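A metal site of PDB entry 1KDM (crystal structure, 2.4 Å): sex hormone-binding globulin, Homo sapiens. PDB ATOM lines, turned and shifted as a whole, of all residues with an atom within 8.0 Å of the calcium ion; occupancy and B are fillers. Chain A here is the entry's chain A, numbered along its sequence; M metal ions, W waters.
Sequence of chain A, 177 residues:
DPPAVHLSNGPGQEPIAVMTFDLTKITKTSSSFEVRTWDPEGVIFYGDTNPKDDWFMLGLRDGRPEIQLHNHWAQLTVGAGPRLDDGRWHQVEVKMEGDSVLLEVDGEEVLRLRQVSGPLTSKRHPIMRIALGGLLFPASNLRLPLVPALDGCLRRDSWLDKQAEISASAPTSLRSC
The side-chain carboxylate (OE2) of Glu 41 sits at hydrogen-bond distance from the backbone NH (N) of Val 147, 2.9 Å away.
N of Asp 151 sits close to OD2 of Asp 39, 2.9 Å away.
The backbone NH (N) of Asp 39 is in hydrogen-bond range of the side-chain hydroxyl (OG1) of Thr 37 (2.9 Å).
The calcium ion is bound by water W2 (2.1 Å).
The calcium ion is bound by the backbone carbonyl oxygen (O) of Glu 41, 2.1 Å away.
O of Ala 149 binds the calcium ion (2.3 Å).
OD2 of Asp 39 is bound to the calcium ion (2.4 Å).
Water W1 binds the calcium ion, at 2.6 Å.
OD1 of Asp 39 is bound to the calcium ion, 2.6 Å away.
Three residues have an atom within 4 Å of the calcium ion: Asp 39, Glu 41 and Ala 149.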
ATOM      1  N   SER A   8     -15.300  22.486   2.164  1.00  0.00           N
ATOM      2  CA  SER A   8     -16.366  22.525   3.151  1.00  0.00           C
ATOM      3  C   SER A   8     -17.528  23.283   2.539  1.00  0.00           C
ATOM      4  O   SER A   8     -17.370  24.017   1.570  1.00  0.00           O
ATOM      5  CB  SER A   8     -16.110  22.950   4.574  1.00  0.00           C
ATOM      6  OG  SER A   8     -15.123  23.922   4.825  1.00  0.00           O
ATOM      7  N   GLN A  13     -20.575  19.994   8.992  1.00  0.00           N
ATOM      8  CA  GLN A  13     -19.298  19.317   8.892  1.00  0.00           C
ATOM      9  C   GLN A  13     -19.312  17.950   8.211  1.00  0.00           C
ATOM     10  O   GLN A  13     -18.347  17.172   8.270  1.00  0.00           O
ATOM     11  CB  GLN A  13     -18.831  19.167  10.351  1.00  0.00           C
ATOM     12  CG  GLN A  13     -18.710  20.600  10.896  1.00  0.00           C
ATOM     13  CD  GLN A  13     -18.169  20.645  12.304  1.00  0.00           C
ATOM     14  OE1 GLN A  13     -18.487  19.732  13.082  1.00  0.00           O
ATOM     15  NE2 GLN A  13     -17.370  21.705  12.479  1.00  0.00           N
ATOM     16  N   THR A  37      -5.178  26.317   1.050  1.00  0.00           N
ATOM     17  CA  THR A  37      -5.934  26.796   2.194  1.00  0.00           C
ATOM     18  C   THR A  37      -5.256  27.913   2.984  1.00  0.00           C
ATOM     19  O   THR A  37      -4.022  27.977   3.055  1.00  0.00           O
ATOM     20  CB  THR A  37      -6.159  25.604   3.152  1.00  0.00           C
ATOM     21  OG1 THR A  37      -7.084  25.941   4.198  1.00  0.00           O
ATOM     22  CG2 THR A  37      -4.901  25.112   3.834  1.00  0.00           C
ATOM     23  N   TRP A  38      -6.018  28.683   3.754  1.00  0.00           N
ATOM     24  CA  TRP A  38      -5.461  29.617   4.713  1.00  0.00           C
ATOM     25  C   TRP A  38      -5.872  29.134   6.105  1.00  0.00           C
ATOM     26  O   TRP A  38      -5.511  29.683   7.133  1.00  0.00           O
ATOM     27  CB  TRP A  38      -5.827  31.098   4.572  1.00  0.00           C
ATOM     28  CG  TRP A  38      -5.528  31.706   3.236  1.00  0.00           C
ATOM     29  CD1 TRP A  38      -6.359  31.658   2.142  1.00  0.00           C
ATOM     30  CD2 TRP A  38      -4.338  32.358   2.807  1.00  0.00           C
ATOM     31  NE1 TRP A  38      -5.774  32.287   1.085  1.00  0.00           N
ATOM     32  CE2 TRP A  38      -4.530  32.726   1.462  1.00  0.00           C
ATOM     33  CE3 TRP A  38      -3.141  32.716   3.426  1.00  0.00           C
ATOM     34  CZ2 TRP A  38      -3.564  33.415   0.711  1.00  0.00           C
ATOM     35  CZ3 TRP A  38      -2.170  33.387   2.707  1.00  0.00           C
ATOM     36  CH2 TRP A  38      -2.401  33.746   1.370  1.00  0.00           C
ATOM     37  N   ASP A  39      -6.635  28.058   6.130  1.00  0.00           N
ATOM     38  CA  ASP A  39      -7.186  27.477   7.351  1.00  0.00           C
ATOM     39  C   ASP A  39      -6.144  26.608   8.033  1.00  0.00           C
ATOM     40  O   ASP A  39      -5.627  25.673   7.457  1.00  0.00           O
ATOM     41  CB  ASP A  39      -8.438  26.700   6.984  1.00  0.00           C
ATOM     42  CG  ASP A  39      -9.356  26.296   8.124  1.00  0.00           C
ATOM     43  OD1 ASP A  39      -8.868  26.410   9.285  1.00  0.00           O
ATOM     44  OD2 ASP A  39     -10.495  25.849   7.808  1.00  0.00           O
ATOM     45  N   PRO A  40      -5.883  26.809   9.327  1.00  0.00           N
ATOM     46  CA  PRO A  40      -4.936  26.012  10.063  1.00  0.00           C
ATOM     47  C   PRO A  40      -5.435  24.630  10.495  1.00  0.00           C
ATOM     48  O   PRO A  40      -4.667  23.870  11.110  1.00  0.00           O
ATOM     49  CB  PRO A  40      -4.662  26.878  11.309  1.00  0.00           C
ATOM     50  CG  PRO A  40      -5.845  27.767  11.486  1.00  0.00           C
ATOM     51  CD  PRO A  40      -6.450  27.975  10.106  1.00  0.00           C
ATOM     52  N   GLU A  41      -6.739  24.403  10.468  1.00  0.00           N
ATOM     53  CA  GLU A  41      -7.268  23.217  11.115  1.00  0.00           C
ATOM     54  C   GLU A  41      -8.484  22.635  10.410  1.00  0.00           C
ATOM     55  O   GLU A  41      -9.367  23.365  10.023  1.00  0.00           O
ATOM     56  CB  GLU A  41      -7.630  23.502  12.593  1.00  0.00           C
ATOM     57  CG  GLU A  41      -8.199  22.291  13.341  1.00  0.00           C
ATOM     58  CD  GLU A  41      -8.428  22.586  14.824  1.00  0.00           C
ATOM     59  OE1 GLU A  41      -7.692  23.283  15.572  1.00  0.00           O
ATOM     60  OE2 GLU A  41      -9.429  22.070  15.348  1.00  0.00           O
ATOM     61  N   GLY A  42      -8.428  21.340  10.132  1.00  0.00           N
ATOM     62  CA  GLY A  42      -9.639  20.707   9.597  1.00  0.00           C
ATOM     63  C   GLY A  42      -9.212  19.400   8.911  1.00  0.00           C
ATOM     64  O   GLY A  42      -8.022  19.044   8.882  1.00  0.00           O
ATOM     65  N   VAL A  43     -10.280  18.728   8.466  1.00  0.00           N
ATOM     66  CA  VAL A  43     -10.114  17.442   7.841  1.00  0.00           C
ATOM     67  C   VAL A  43      -9.913  17.550   6.337  1.00  0.00           C
ATOM     68  O   VAL A  43     -10.672  18.271   5.680  1.00  0.00           O
ATOM     69  CB  VAL A  43     -11.300  16.511   8.146  1.00  0.00           C
ATOM     70  CG1 VAL A  43     -11.170  15.229   7.317  1.00  0.00           C
ATOM     71  CG2 VAL A  43     -11.324  16.222   9.648  1.00  0.00           C
ATOM     72  N   LEU A  60      -5.214  18.892   8.861  1.00  0.00           N
ATOM     73  CA  LEU A  60      -4.287  19.894   9.357  1.00  0.00           C
ATOM     74  C   LEU A  60      -4.600  20.230  10.813  1.00  0.00           C
ATOM     75  O   LEU A  60      -5.775  20.338  11.202  1.00  0.00           O
ATOM     76  CB  LEU A  60      -4.359  21.208   8.587  1.00  0.00           C
ATOM     77  CG  LEU A  60      -4.086  21.098   7.081  1.00  0.00           C
ATOM     78  CD1 LEU A  60      -4.161  22.445   6.389  1.00  0.00           C
ATOM     79  CD2 LEU A  60      -2.725  20.383   6.910  1.00  0.00           C
ATOM     80  N   LEU A 146     -10.612  17.622  16.766  1.00  0.00           N
ATOM     81  CA  LEU A 146     -10.348  18.843  16.030  1.00  0.00           C
ATOM     82  C   LEU A 146     -11.689  19.283  15.444  1.00  0.00           C
ATOM     83  O   LEU A 146     -12.587  18.431  15.455  1.00  0.00           O
ATOM     84  CB  LEU A 146      -9.243  18.656  15.038  1.00  0.00           C
ATOM     85  CG  LEU A 146      -9.284  17.679  13.888  1.00  0.00           C
ATOM     86  CD1 LEU A 146     -10.534  17.795  13.038  1.00  0.00           C
ATOM     87  CD2 LEU A 146      -8.052  17.949  13.017  1.00  0.00           C
ATOM     88  N   VAL A 147     -11.838  20.555  15.133  1.00  0.00           N
ATOM     89  CA  VAL A 147     -13.033  21.028  14.438  1.00  0.00           C
ATOM     90  C   VAL A 147     -12.813  20.705  12.950  1.00  0.00           C
ATOM     91  O   VAL A 147     -11.829  21.131  12.362  1.00  0.00           O
ATOM     92  CB  VAL A 147     -13.257  22.536  14.650  1.00  0.00           C
ATOM     93  CG1 VAL A 147     -14.571  22.955  13.969  1.00  0.00           C
ATOM     94  CG2 VAL A 147     -13.270  22.948  16.109  1.00  0.00           C
ATOM     95  N   PRO A 148     -13.540  19.755  12.423  1.00  0.00           N
ATOM     96  CA  PRO A 148     -13.372  19.240  11.084  1.00  0.00           C
ATOM     97  C   PRO A 148     -13.387  20.208   9.918  1.00  0.00           C
ATOM     98  O   PRO A 148     -12.654  19.937   8.955  1.00  0.00           O
ATOM     99  CB  PRO A 148     -14.561  18.294  10.882  1.00  0.00           C
ATOM    100  CG  PRO A 148     -15.038  17.955  12.267  1.00  0.00           C
ATOM    101  CD  PRO A 148     -14.730  19.149  13.115  1.00  0.00           C
ATOM    102  N   ALA A 149     -14.146  21.291   9.938  1.00  0.00           N
ATOM    103  CA  ALA A 149     -14.278  22.115   8.739  1.00  0.00           C
ATOM    104  C   ALA A 149     -12.935  22.704   8.288  1.00  0.00           C
ATOM    105  O   ALA A 149     -12.205  23.419   9.004  1.00  0.00           O
ATOM    106  CB  ALA A 149     -15.266  23.267   9.011  1.00  0.00           C
ATOM    107  N   LEU A 150     -12.636  22.460   7.027  1.00  0.00           N
ATOM    108  CA  LEU A 150     -11.442  22.953   6.360  1.00  0.00           C
ATOM    109  C   LEU A 150     -11.936  23.762   5.160  1.00  0.00           C
ATOM    110  O   LEU A 150     -12.503  23.337   4.152  1.00  0.00           O
ATOM    111  CB  LEU A 150     -10.471  21.871   5.948  1.00  0.00           C
ATOM    112  CG  LEU A 150      -9.006  22.112   5.572  1.00  0.00           C
ATOM    113  CD1 LEU A 150      -8.891  22.554   4.120  1.00  0.00           C
ATOM    114  CD2 LEU A 150      -8.320  23.145   6.453  1.00  0.00           C
ATOM    115  N   ASP A 151     -11.751  25.058   5.312  1.00  0.00           N
ATOM    116  CA  ASP A 151     -12.145  26.031   4.309  1.00  0.00           C
ATOM    117  C   ASP A 151     -10.994  26.074   3.341  1.00  0.00           C
ATOM    118  O   ASP A 151     -10.017  26.796   3.470  1.00  0.00           O
ATOM    119  CB  ASP A 151     -12.375  27.332   5.069  1.00  0.00           C
ATOM    120  CG  ASP A 151     -12.823  28.466   4.165  1.00  0.00           C
ATOM    121  OD1 ASP A 151     -12.132  28.722   3.166  1.00  0.00           O
ATOM    122  OD2 ASP A 151     -13.861  29.092   4.493  1.00  0.00           O
ATOM    123  N   GLY A 152     -11.039  25.190   2.357  1.00  0.00           N
ATOM    124  CA  GLY A 152      -9.942  25.068   1.417  1.00  0.00           C
ATOM    125  C   GLY A 152     -10.423  24.523   0.095  1.00  0.00           C
ATOM    126  O   GLY A 152     -11.632  24.358  -0.122  1.00  0.00           O
HETATM  127 CA    CA M   1     -10.844  24.927  10.032  1.00  0.00          CA
HETATM  128  O   HOH W   1     -10.155  26.570  11.872  1.00  0.00           O
HETATM  129  O   HOH W   2     -11.467  23.800  11.751  1.00  0.00           O
